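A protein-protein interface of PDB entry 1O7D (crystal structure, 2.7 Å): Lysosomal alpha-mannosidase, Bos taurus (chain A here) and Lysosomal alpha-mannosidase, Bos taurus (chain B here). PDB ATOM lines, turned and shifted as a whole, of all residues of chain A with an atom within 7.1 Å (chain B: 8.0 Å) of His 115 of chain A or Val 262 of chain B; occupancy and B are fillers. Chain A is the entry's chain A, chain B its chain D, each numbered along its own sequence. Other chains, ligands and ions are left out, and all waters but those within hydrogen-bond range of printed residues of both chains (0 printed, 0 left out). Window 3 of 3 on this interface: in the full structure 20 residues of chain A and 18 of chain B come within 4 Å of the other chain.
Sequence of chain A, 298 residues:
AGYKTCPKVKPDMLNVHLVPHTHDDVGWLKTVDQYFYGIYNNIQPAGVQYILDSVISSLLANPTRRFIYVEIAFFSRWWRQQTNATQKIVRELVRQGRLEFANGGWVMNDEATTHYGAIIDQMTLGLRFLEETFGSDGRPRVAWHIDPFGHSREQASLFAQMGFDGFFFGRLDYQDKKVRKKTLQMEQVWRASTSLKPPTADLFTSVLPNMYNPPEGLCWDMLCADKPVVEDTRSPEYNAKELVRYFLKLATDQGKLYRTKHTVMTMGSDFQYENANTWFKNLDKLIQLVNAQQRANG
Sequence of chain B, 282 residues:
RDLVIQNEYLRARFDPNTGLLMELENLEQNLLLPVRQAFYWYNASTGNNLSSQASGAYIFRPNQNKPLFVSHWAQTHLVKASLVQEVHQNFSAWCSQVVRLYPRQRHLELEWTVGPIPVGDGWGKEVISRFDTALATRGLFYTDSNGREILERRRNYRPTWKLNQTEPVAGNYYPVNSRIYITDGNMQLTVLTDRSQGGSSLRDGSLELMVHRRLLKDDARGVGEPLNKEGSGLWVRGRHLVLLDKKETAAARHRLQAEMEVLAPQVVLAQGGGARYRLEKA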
ATOM      1  N   ASP A 110       9.464 -22.479  36.911  1.00  0.00           N
ATOM      2  CA  ASP A 110       8.514 -21.514  37.449  1.00  0.00           C
ATOM      3  C   ASP A 110       7.130 -22.153  37.439  1.00  0.00           C
ATOM      4  O   ASP A 110       6.897 -23.090  36.689  1.00  0.00           O
ATOM      5  CB  ASP A 110       8.500 -20.269  36.572  1.00  0.00           C
ATOM      6  CG  ASP A 110       7.418 -19.326  36.960  1.00  0.00           C
ATOM      7  OD1 ASP A 110       7.524 -18.737  38.067  1.00  0.00           O
ATOM      8  OD2 ASP A 110       6.462 -19.199  36.170  1.00  0.00           O
ATOM      9  N   ALA A 112       3.946 -20.183  37.344  1.00  0.00           N
ATOM     10  CA  ALA A 112       2.835 -19.369  36.852  1.00  0.00           C
ATOM     11  C   ALA A 112       2.707 -19.298  35.330  1.00  0.00           C
ATOM     12  O   ALA A 112       1.602 -19.279  34.795  1.00  0.00           O
ATOM     13  CB  ALA A 112       2.930 -17.955  37.437  1.00  0.00           C
ATOM     14  N   THR A 113       3.837 -19.283  34.637  1.00  0.00           N
ATOM     15  CA  THR A 113       3.832 -19.167  33.195  1.00  0.00           C
ATOM     16  C   THR A 113       4.194 -20.417  32.405  1.00  0.00           C
ATOM     17  O   THR A 113       4.150 -20.408  31.178  1.00  0.00           O
ATOM     18  CB  THR A 113       4.758 -18.037  32.784  1.00  0.00           C
ATOM     19  OG1 THR A 113       6.058 -18.253  33.353  1.00  0.00           O
ATOM     20  CG2 THR A 113       4.187 -16.696  33.270  1.00  0.00           C
ATOM     21  N   THR A 114       4.538 -21.494  33.089  1.00  0.00           N
ATOM     22  CA  THR A 114       4.895 -22.725  32.403  1.00  0.00           C
ATOM     23  C   THR A 114       3.698 -23.570  31.993  1.00  0.00           C
ATOM     24  O   THR A 114       2.662 -23.558  32.648  1.00  0.00           O
ATOM     25  CB  THR A 114       5.779 -23.576  33.269  1.00  0.00           C
ATOM     26  OG1 THR A 114       5.195 -23.669  34.574  1.00  0.00           O
ATOM     27  CG2 THR A 114       7.156 -22.962  33.367  1.00  0.00           C
ATOM     28  N   HIS A 115       3.865 -24.303  30.897  1.00  0.00           N
ATOM     29  CA  HIS A 115       2.847 -25.180  30.334  1.00  0.00           C
ATOM     30  C   HIS A 115       3.063 -26.533  30.982  1.00  0.00           C
ATOM     31  O   HIS A 115       4.195 -26.990  31.031  1.00  0.00           O
ATOM     32  CB  HIS A 115       3.068 -25.279  28.821  1.00  0.00           C
ATOM     33  CG  HIS A 115       2.166 -26.252  28.134  1.00  0.00           C
ATOM     34  ND1 HIS A 115       0.798 -26.101  28.094  1.00  0.00           N
ATOM     35  CD2 HIS A 115       2.440 -27.393  27.464  1.00  0.00           C
ATOM     36  CE1 HIS A 115       0.265 -27.109  27.429  1.00  0.00           C
ATOM     37  NE2 HIS A 115       1.240 -27.906  27.035  1.00  0.00           N
ATOM     38  N   TYR A 116       2.011 -27.187  31.467  1.00  0.00           N
ATOM     39  CA  TYR A 116       2.202 -28.482  32.129  1.00  0.00           C
ATOM     40  C   TYR A 116       3.046 -29.475  31.309  1.00  0.00           C
ATOM     41  O   TYR A 116       3.863 -30.212  31.859  1.00  0.00           O
ATOM     42  CB  TYR A 116       0.845 -29.102  32.478  1.00  0.00           C
ATOM     43  CG  TYR A 116       0.177 -29.821  31.341  1.00  0.00           C
ATOM     44  CD1 TYR A 116       0.508 -31.143  31.031  1.00  0.00           C
ATOM     45  CD2 TYR A 116      -0.751 -29.176  30.547  1.00  0.00           C
ATOM     46  CE1 TYR A 116      -0.073 -31.797  29.947  1.00  0.00           C
ATOM     47  CE2 TYR A 116      -1.336 -29.813  29.466  1.00  0.00           C
ATOM     48  CZ  TYR A 116      -0.998 -31.121  29.161  1.00  0.00           C
ATOM     49  OH  TYR A 116      -1.581 -31.735  28.059  1.00  0.00           O
ATOM     50  N   GLY A 117       2.858 -29.472  29.992  1.00  0.00           N
ATOM     51  CA  GLY A 117       3.589 -30.383  29.134  1.00  0.00           C
ATOM     52  C   GLY A 117       5.060 -30.067  29.076  1.00  0.00           C
ATOM     53  O   GLY A 117       5.887 -30.961  29.011  1.00  0.00           O
ATOM     54  N   ALA A 118       5.384 -28.782  29.098  1.00  0.00           N
ATOM     55  CA  ALA A 118       6.763 -28.349  29.037  1.00  0.00           C
ATOM     56  C   ALA A 118       7.467 -28.635  30.354  1.00  0.00           C
ATOM     57  O   ALA A 118       8.655 -28.955  30.379  1.00  0.00           O
ATOM     58  CB  ALA A 118       6.803 -26.884  28.713  1.00  0.00           C
ATOM     59  N   ILE A 119       6.730 -28.516  31.450  1.00  0.00           N
ATOM     60  CA  ILE A 119       7.279 -28.791  32.766  1.00  0.00           C
ATOM     61  C   ILE A 119       7.698 -30.257  32.829  1.00  0.00           C
ATOM     62  O   ILE A 119       8.682 -30.612  33.460  1.00  0.00           O
ATOM     63  CB  ILE A 119       6.221 -28.526  33.855  1.00  0.00           C
ATOM     64  CG1 ILE A 119       5.929 -27.031  33.923  1.00  0.00           C
ATOM     65  CG2 ILE A 119       6.691 -29.050  35.203  1.00  0.00           C
ATOM     66  CD1 ILE A 119       4.684 -26.699  34.728  1.00  0.00           C
ATOM     67  N   ILE A 120       6.939 -31.113  32.167  1.00  0.00           N
ATOM     68  CA  ILE A 120       7.251 -32.530  32.165  1.00  0.00           C
ATOM     69  C   ILE A 120       8.510 -32.836  31.351  1.00  0.00           C
ATOM     70  O   ILE A 120       9.396 -33.558  31.816  1.00  0.00           O
ATOM     71  CB  ILE A 120       6.062 -33.335  31.625  1.00  0.00           C
ATOM     72  CG1 ILE A 120       4.820 -33.022  32.463  1.00  0.00           C
ATOM     73  CG2 ILE A 120       6.372 -34.827  31.660  1.00  0.00           C
ATOM     74  CD1 ILE A 120       3.556 -33.709  31.962  1.00  0.00           C
ATOM     75  N   ASP A 121       8.599 -32.300  30.136  1.00  0.00           N
ATOM     76  CA  ASP A 121       9.793 -32.545  29.335  1.00  0.00           C
ATOM     77  C   ASP A 121      11.026 -32.134  30.140  1.00  0.00           C
ATOM     78  O   ASP A 121      12.028 -32.855  30.178  1.00  0.00           O
ATOM     79  CB  ASP A 121       9.747 -31.762  28.014  1.00  0.00           C
ATOM     80  CG  ASP A 121       8.629 -32.248  27.081  1.00  0.00           C
ATOM     81  OD1 ASP A 121       8.524 -33.467  26.851  1.00  0.00           O
ATOM     82  OD2 ASP A 121       7.850 -31.421  26.555  1.00  0.00           O
ATOM     83  N   LEU A 158       1.420 -32.749  39.266  1.00  0.00           N
ATOM     84  CA  LEU A 158       2.486 -33.295  38.443  1.00  0.00           C
ATOM     85  C   LEU A 158       3.529 -34.023  39.267  1.00  0.00           C
ATOM     86  O   LEU A 158       3.923 -35.144  38.927  1.00  0.00           O
ATOM     87  CB  LEU A 158       3.143 -32.177  37.627  1.00  0.00           C
ATOM     88  CG  LEU A 158       2.702 -31.966  36.166  1.00  0.00           C
ATOM     89  CD1 LEU A 158       1.222 -32.258  35.955  1.00  0.00           C
ATOM     90  CD2 LEU A 158       3.024 -30.547  35.780  1.00  0.00           C
ATOM     91  N   ASP B 144      -7.169 -21.311  34.177  1.00  0.00           N
ATOM     92  CA  ASP B 144      -6.580 -22.630  34.047  1.00  0.00           C
ATOM     93  C   ASP B 144      -5.222 -22.652  34.737  1.00  0.00           C
ATOM     94  O   ASP B 144      -4.469 -21.692  34.678  1.00  0.00           O
ATOM     95  CB  ASP B 144      -6.436 -23.016  32.562  1.00  0.00           C
ATOM     96  CG  ASP B 144      -5.413 -22.159  31.813  1.00  0.00           C
ATOM     97  OD1 ASP B 144      -5.731 -21.001  31.443  1.00  0.00           O
ATOM     98  OD2 ASP B 144      -4.281 -22.655  31.594  1.00  0.00           O
ATOM     99  N   SER B 145      -4.919 -23.749  35.413  1.00  0.00           N
ATOM    100  CA  SER B 145      -3.632 -23.876  36.082  1.00  0.00           C
ATOM    101  C   SER B 145      -2.689 -24.599  35.132  1.00  0.00           C
ATOM    102  O   SER B 145      -2.832 -25.788  34.886  1.00  0.00           O
ATOM    103  CB  SER B 145      -3.777 -24.669  37.395  1.00  0.00           C
ATOM    104  OG  SER B 145      -2.546 -24.824  38.102  1.00  0.00           O
ATOM    105  N   ASN B 146      -1.727 -23.873  34.589  1.00  0.00           N
ATOM    106  CA  ASN B 146      -0.774 -24.473  33.665  1.00  0.00           C
ATOM    107  C   ASN B 146      -1.441 -25.284  32.562  1.00  0.00           C
ATOM    108  O   ASN B 146      -0.889 -26.273  32.085  1.00  0.00           O
ATOM    109  CB  ASN B 146       0.217 -25.347  34.426  1.00  0.00           C
ATOM    110  CG  ASN B 146       1.047 -24.556  35.397  1.00  0.00           C
ATOM    111  OD1 ASN B 146       1.628 -23.531  35.040  1.00  0.00           O
ATOM    112  ND2 ASN B 146       1.109 -25.021  36.633  1.00  0.00           N
ATOM    113  N   GLY B 147      -2.644 -24.861  32.174  1.00  0.00           N
ATOM    114  CA  GLY B 147      -3.380 -25.510  31.090  1.00  0.00           C
ATOM    115  C   GLY B 147      -4.084 -26.827  31.379  1.00  0.00           C
ATOM    116  O   GLY B 147      -4.357 -27.574  30.455  1.00  0.00           O
ATOM    117  N   ARG B 148      -4.395 -27.122  32.642  1.00  0.00           N
ATOM    118  CA  ARG B 148      -5.061 -28.387  32.969  1.00  0.00           C
ATOM    119  C   ARG B 148      -6.394 -28.208  33.660  1.00  0.00           C
ATOM    120  O   ARG B 148      -7.386 -27.863  33.013  1.00  0.00           O
ATOM    121  CB  ARG B 148      -4.162 -29.275  33.829  1.00  0.00           C
ATOM    122  CG  ARG B 148      -2.885 -29.675  33.126  1.00  0.00           C
ATOM    123  CD  ARG B 148      -2.525 -31.115  33.407  1.00  0.00           C
ATOM    124  NE  ARG B 148      -3.516 -32.025  32.852  1.00  0.00           N
ATOM    125  CZ  ARG B 148      -3.521 -33.341  33.046  1.00  0.00           C
ATOM    126  NH1 ARG B 148      -2.589 -33.926  33.785  1.00  0.00           N
ATOM    127  NH2 ARG B 148      -4.467 -34.080  32.492  1.00  0.00           N
ATOM    128  N   ASN B 177      -2.629 -19.279  31.731  1.00  0.00           N
ATOM    129  CA  ASN B 177      -1.737 -19.848  30.734  1.00  0.00           C
ATOM    130  C   ASN B 177      -2.388 -20.263  29.431  1.00  0.00           C
ATOM    131  O   ASN B 177      -1.698 -20.382  28.410  1.00  0.00           O
ATOM    132  CB  ASN B 177      -0.999 -21.067  31.302  1.00  0.00           C
ATOM    133  CG  ASN B 177      -0.180 -20.734  32.526  1.00  0.00           C
ATOM    134  OD1 ASN B 177       0.268 -19.605  32.704  1.00  0.00           O
ATOM    135  ND2 ASN B 177       0.032 -21.719  33.371  1.00  0.00           N
ATOM    136  N   SER B 178      -3.698 -20.491  29.443  1.00  0.00           N
ATOM    137  CA  SER B 178      -4.382 -20.935  28.226  1.00  0.00           C
ATOM    138  C   SER B 178      -5.735 -20.285  28.097  1.00  0.00           C
ATOM    139  O   SER B 178      -6.145 -19.890  27.006  1.00  0.00           O
ATOM    140  CB  SER B 178      -4.606 -22.456  28.240  1.00  0.00           C
ATOM    141  OG  SER B 178      -3.433 -23.183  28.576  1.00  0.00           O
ATOM    142  N   ARG B 179      -6.426 -20.176  29.225  1.00  0.00           N
ATOM    143  CA  ARG B 179      -7.768 -19.637  29.209  1.00  0.00           C
ATOM    144  C   ARG B 179      -8.228 -18.969  30.489  1.00  0.00           C
ATOM    145  O   ARG B 179      -7.551 -18.993  31.517  1.00  0.00           O
ATOM    146  CB  ARG B 179      -8.750 -20.759  28.867  1.00  0.00           C
ATOM    147  CG  ARG B 179      -8.863 -21.828  29.952  1.00  0.00           C
ATOM    148  CD  ARG B 179      -8.970 -23.209  29.367  1.00  0.00           C
ATOM    149  NE  ARG B 179      -7.655 -23.724  29.026  1.00  0.00           N
ATOM    150  CZ  ARG B 179      -7.434 -24.932  28.518  1.00  0.00           C
ATOM    151  NH1 ARG B 179      -8.443 -25.772  28.282  1.00  0.00           N
ATOM    152  NH2 ARG B 179      -6.188 -25.299  28.255  1.00  0.00           N
ATOM    153  N   THR B 193      -5.680 -17.929  25.052  1.00  0.00           N
ATOM    154  CA  THR B 193      -4.480 -17.150  24.763  1.00  0.00           C
ATOM    155  C   THR B 193      -3.442 -17.957  23.996  1.00  0.00           C
ATOM    156  O   THR B 193      -3.500 -19.183  23.948  1.00  0.00           O
ATOM    157  CB  THR B 193      -3.810 -16.682  26.039  1.00  0.00           C
ATOM    158  OG1 THR B 193      -3.211 -17.808  26.686  1.00  0.00           O
ATOM    159  CG2 THR B 193      -4.831 -16.052  26.979  1.00  0.00           C
ATOM    160  N   ASP B 194      -2.475 -17.263  23.409  1.00  0.00           N
ATOM    161  CA  ASP B 194      -1.416 -17.917  22.661  1.00  0.00           C
ATOM    162  C   ASP B 194      -0.138 -18.000  23.486  1.00  0.00           C
ATOM    163  O   ASP B 194       0.852 -18.579  23.056  1.00  0.00           O
ATOM    164  CB  ASP B 194      -1.129 -17.157  21.367  1.00  0.00           C
ATOM    165  CG  ASP B 194      -0.765 -15.688  21.603  1.00  0.00           C
ATOM    166  OD1 ASP B 194      -0.284 -15.317  22.697  1.00  0.00           O
ATOM    167  OD2 ASP B 194      -0.944 -14.898  20.660  1.00  0.00           O
ATOM    168  N   ARG B 195      -0.168 -17.399  24.668  1.00  0.00           N
ATOM    169  CA  ARG B 195       0.973 -17.390  25.573  1.00  0.00           C
ATOM    170  C   ARG B 195       0.420 -17.102  26.966  1.00  0.00           C
ATOM    171  O   ARG B 195      -0.720 -16.654  27.107  1.00  0.00           O
ATOM    172  CB  ARG B 195       1.951 -16.289  25.173  1.00  0.00           C
ATOM    173  CG  ARG B 195       1.429 -14.881  25.434  1.00  0.00           C
ATOM    174  CD  ARG B 195       2.248 -13.870  24.699  1.00  0.00           C
ATOM    175  NE  ARG B 195       1.880 -13.817  23.294  1.00  0.00           N
ATOM    176  CZ  ARG B 195       2.591 -13.190  22.370  1.00  0.00           C
ATOM    177  NH1 ARG B 195       3.711 -12.565  22.696  1.00  0.00           N
ATOM    178  NH2 ARG B 195       2.181 -13.182  21.121  1.00  0.00           N
ATOM    179  N   SER B 196       1.213 -17.351  27.999  1.00  0.00           N
ATOM    180  CA  SER B 196       0.722 -17.100  29.348  1.00  0.00           C
ATOM    181  C   SER B 196       0.619 -15.601  29.610  1.00  0.00           C
ATOM    182  O   SER B 196       1.495 -14.837  29.213  1.00  0.00           O
ATOM    183  CB  SER B 196       1.623 -17.781  30.393  1.00  0.00           C
ATOM    184  OG  SER B 196       2.977 -17.397  30.275  1.00  0.00           O
ATOM    185  N   ARG B 239      -2.608 -13.383  19.574  1.00  0.00           N
ATOM    186  CA  ARG B 239      -4.024 -13.674  19.318  1.00  0.00           C
ATOM    187  C   ARG B 239      -4.787 -14.052  20.591  1.00  0.00           C
ATOM    188  O   ARG B 239      -4.201 -14.505  21.573  1.00  0.00           O
ATOM    189  CB  ARG B 239      -4.175 -14.810  18.295  1.00  0.00           C
ATOM    190  CG  ARG B 239      -3.243 -14.706  17.092  1.00  0.00           C
ATOM    191  CD  ARG B 239      -3.669 -15.609  15.943  1.00  0.00           C
ATOM    192  NE  ARG B 239      -4.028 -16.957  16.374  1.00  0.00           N
ATOM    193  CZ  ARG B 239      -3.221 -17.804  17.020  1.00  0.00           C
ATOM    194  NH1 ARG B 239      -1.971 -17.472  17.337  1.00  0.00           N
ATOM    195  NH2 ARG B 239      -3.677 -19.001  17.357  1.00  0.00           N
ATOM    196  N   LEU B 256     -11.115 -28.770  23.585  1.00  0.00           N
ATOM    197  CA  LEU B 256     -10.690 -29.160  22.242  1.00  0.00           C
ATOM    198  C   LEU B 256      -9.995 -28.101  21.399  1.00  0.00           C
ATOM    199  O   LEU B 256      -9.100 -28.427  20.617  1.00  0.00           O
ATOM    200  CB  LEU B 256     -11.877 -29.705  21.450  1.00  0.00           C
ATOM    201  CG  LEU B 256     -12.514 -30.958  22.035  1.00  0.00           C
ATOM    202  CD1 LEU B 256     -13.679 -31.389  21.181  1.00  0.00           C
ATOM    203  CD2 LEU B 256     -11.466 -32.055  22.119  1.00  0.00           C
ATOM    204  N   GLN B 257     -10.407 -26.846  21.521  1.00  0.00           N
ATOM    205  CA  GLN B 257      -9.768 -25.814  20.720  1.00  0.00           C
ATOM    206  C   GLN B 257      -8.463 -25.398  21.377  1.00  0.00           C
ATOM    207  O   GLN B 257      -7.499 -25.025  20.696  1.00  0.00           O
ATOM    208  CB  GLN B 257     -10.663 -24.589  20.583  1.00  0.00           C
ATOM    209  CG  GLN B 257     -10.012 -23.513  19.736  1.00  0.00           C
ATOM    210  CD  GLN B 257     -10.155 -23.789  18.257  1.00  0.00           C
ATOM    211  OE1 GLN B 257     -11.270 -23.731  17.715  1.00  0.00           O
ATOM    212  NE2 GLN B 257      -9.039 -24.102  17.589  1.00  0.00           N
ATOM    213  N   ALA B 258      -8.452 -25.458  22.710  1.00  0.00           N
ATOM    214  CA  ALA B 258      -7.275 -25.084  23.475  1.00  0.00           C
ATOM    215  C   ALA B 258      -6.162 -26.032  23.076  1.00  0.00           C
ATOM    216  O   ALA B 258      -5.002 -25.624  22.945  1.00  0.00           O
ATOM    217  CB  ALA B 258      -7.554 -25.178  24.964  1.00  0.00           C
ATOM    218  N   GLU B 259      -6.505 -27.297  22.868  1.00  0.00           N
ATOM    219  CA  GLU B 259      -5.470 -28.234  22.461  1.00  0.00           C
ATOM    220  C   GLU B 259      -5.055 -27.996  21.009  1.00  0.00           C
ATOM    221  O   GLU B 259      -3.897 -28.201  20.659  1.00  0.00           O
ATOM    222  CB  GLU B 259      -5.914 -29.686  22.645  1.00  0.00           C
ATOM    223  CG  GLU B 259      -7.120 -30.073  21.868  1.00  0.00           C
ATOM    224  CD  GLU B 259      -7.069 -31.535  21.377  1.00  0.00           C
ATOM    225  OE1 GLU B 259      -6.168 -32.326  21.817  1.00  0.00           O
ATOM    226  OE2 GLU B 259      -7.958 -31.877  20.542  1.00  0.00           O
ATOM    227  N   MET B 260      -5.982 -27.559  20.162  1.00  0.00           N
ATOM    228  CA  MET B 260      -5.635 -27.305  18.769  1.00  0.00           C
ATOM    229  C   MET B 260      -4.748 -26.077  18.693  1.00  0.00           C
ATOM    230  O   MET B 260      -4.062 -25.846  17.702  1.00  0.00           O
ATOM    231  CB  MET B 260      -6.885 -27.078  17.928  1.00  0.00           C
ATOM    232  CG  MET B 260      -7.732 -28.311  17.736  1.00  0.00           C
ATOM    233  SD  MET B 260      -9.073 -28.021  16.541  1.00  0.00           S
ATOM    234  CE  MET B 260     -10.478 -27.636  17.618  1.00  0.00           C
ATOM    235  N   GLU B 261      -4.758 -25.311  19.775  1.00  0.00           N
ATOM    236  CA  GLU B 261      -3.997 -24.075  19.910  1.00  0.00           C
ATOM    237  C   GLU B 261      -2.519 -24.276  20.265  1.00  0.00           C
ATOM    238  O   GLU B 261      -1.645 -23.608  19.718  1.00  0.00           O
ATOM    239  CB  GLU B 261      -4.681 -23.211  20.973  1.00  0.00           C
ATOM    240  CG  GLU B 261      -4.166 -21.798  21.107  1.00  0.00           C
ATOM    241  CD  GLU B 261      -4.050 -21.109  19.777  1.00  0.00           C
ATOM    242  OE1 GLU B 261      -5.006 -21.209  18.968  1.00  0.00           O
ATOM    243  OE2 GLU B 261      -2.999 -20.471  19.548  1.00  0.00           O
ATOM    244  N   VAL B 262      -2.244 -25.178  21.202  1.00  0.00           N
ATOM    245  CA  VAL B 262      -0.872 -25.466  21.605  1.00  0.00           C
ATOM    246  C   VAL B 262      -0.202 -26.484  20.656  1.00  0.00           C
ATOM    247  O   VAL B 262       0.967 -26.330  20.289  1.00  0.00           O
ATOM    248  CB  VAL B 262      -0.844 -25.992  23.051  1.00  0.00           C
ATOM    249  CG1 VAL B 262       0.591 -26.302  23.490  1.00  0.00           C
ATOM    250  CG2 VAL B 262      -1.446 -24.944  23.962  1.00  0.00           C
ATOM    251  N   LEU B 263      -0.942 -27.520  20.269  1.00  0.00           N
ATOM    252  CA  LEU B 263      -0.429 -28.536  19.355  1.00  0.00           C
ATOM    253  C   LEU B 263      -0.973 -28.214  17.979  1.00  0.00           C
ATOM    254  O   LEU B 263      -1.716 -28.998  17.393  1.00  0.00           O
ATOM    255  CB  LEU B 263      -0.891 -29.915  19.791  1.00  0.00           C
ATOM    256  CG  LEU B 263      -0.162 -30.402  21.033  1.00  0.00           C
ATOM    257  CD1 LEU B 263      -0.637 -31.798  21.400  1.00  0.00           C
ATOM    258  CD2 LEU B 263       1.339 -30.384  20.743  1.00  0.00           C
ATOM    259  N   ALA B 264      -0.606 -27.041  17.478  1.00  0.00           N
ATOM    260  CA  ALA B 264      -1.075 -26.571  16.189  1.00  0.00           C
ATOM    261  C   ALA B 264      -0.337 -27.218  15.024  1.00  0.00           C
ATOM    262  O   ALA B 264       0.647 -27.925  15.216  1.00  0.00           O
ATOM    263  CB  ALA B 264      -0.943 -25.071  16.132  1.00  0.00           C
ATOM    264  N   PRO B 265      -0.813 -26.988  13.791  1.00  0.00           N
ATOM    265  CA  PRO B 265      -0.135 -27.594  12.648  1.00  0.00           C
ATOM    266  C   PRO B 265       1.153 -26.873  12.250  1.00  0.00           C
ATOM    267  O   PRO B 265       1.279 -25.668  12.450  1.00  0.00           O
ATOM    268  CB  PRO B 265      -1.218 -27.581  11.573  1.00  0.00           C
ATOM    269  CG  PRO B 265      -1.996 -26.386  11.902  1.00  0.00           C
ATOM    270  CD  PRO B 265      -2.100 -26.396  13.390  1.00  0.00           C
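The side-chain amide oxygen (OD1) of Asn 177 of chain B sits close to the backbone carbonyl oxygen (O) of Ala 112 of chain A (2.5 Å).
The side-chain hydroxyl (OG) of Ser 196 of chain B sits close to the backbone carbonyl oxygen (O) of Thr 113 of chain A (3.4 Å).
The backbone carbonyl oxygen of Thr 114 of chain A lies close to the side-chain amide oxygen of Asn 146 of chain B.
The side-chain amide nitrogen (ND2) of Asn 177 of chain B sits at hydrogen-bond distance from the backbone carbonyl oxygen (O) of Thr 114 of chain A (3.3 Å).
The backbone NH of Tyr 116 of chain A lies within hydrogen-bond range of the backbone carbonyl oxygen of Asn 146 of chain B.
OD2 of Asp 110 of chain A lies within hydrogen-bond range of N of Ala 112 of chain A.
OG1 of Thr 113 of chain A is in hydrogen-bond range of OD2 of Asp 110 of chain A (3.0 Å).
The side-chain hydroxyl (OG1) of Thr 114 of chain A lies within hydrogen-bond range of the backbone carbonyl oxygen (O) of Asp 110 of chain A.
N of Gly 147 of chain B sits at hydrogen-bond distance from OD2 of Asp 144 of chain B (2.8 Å).
The side-chain amide nitrogen of Asn 177 of chain B lies close to the side-chain amide oxygen of Asn 146 of chain B (2.9 Å).
OG1 of Thr 193 of chain B sits at hydrogen-bond distance from O of Asn 177 of chain B, at 3.4 Å.
Asn 177 of chain B touches Thr 113 of chain A.
NE2 of His 115 of chain A touches CG1 of Val 262 of chain B, 3.9 Å away.
Tyr 116 of chain A touches Gly 147 of chain B.
CG of Arg 148 of chain B touches CD2 of Tyr 116 of chain A, 3.4 Å away.
Of the printed residues of chain B, Thr 114 of chain A touches Asn 146 and Asn 177.
His 115 of chain A touches just one residue of chain B: Val 262.
Of the printed residues of chain B, Tyr 116 of chain A touches Asn 146, Gly 147 and Arg 148.
Of the printed residues of chain A, Ser 196 of chain B touches Thr 113 (3.1 Å).
Val 262 of chain B touches one residue of chain A.
The nearest printed residue of chain A that does not touch Val 262 of chain B is Tyr 116 of chain A (7.2 Å).
Hydrophobic or aromatic side chains of chain B that line the printed part of chain A: Val 262.
Of the 12 printed residues of chain A, 5 touch a printed residue of chain B.
Printed residues of chain A that touch a printed residue of chain B: Ala 112, Thr 113, Thr 114, His 115 and Tyr 116.
Among the printed residues, 9 pairs touch across the chains.
Among the printed residues, no Asp or Glu carboxylate lies within 4 Å of a Lys or Arg side-chain nitrogen of the other chain.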
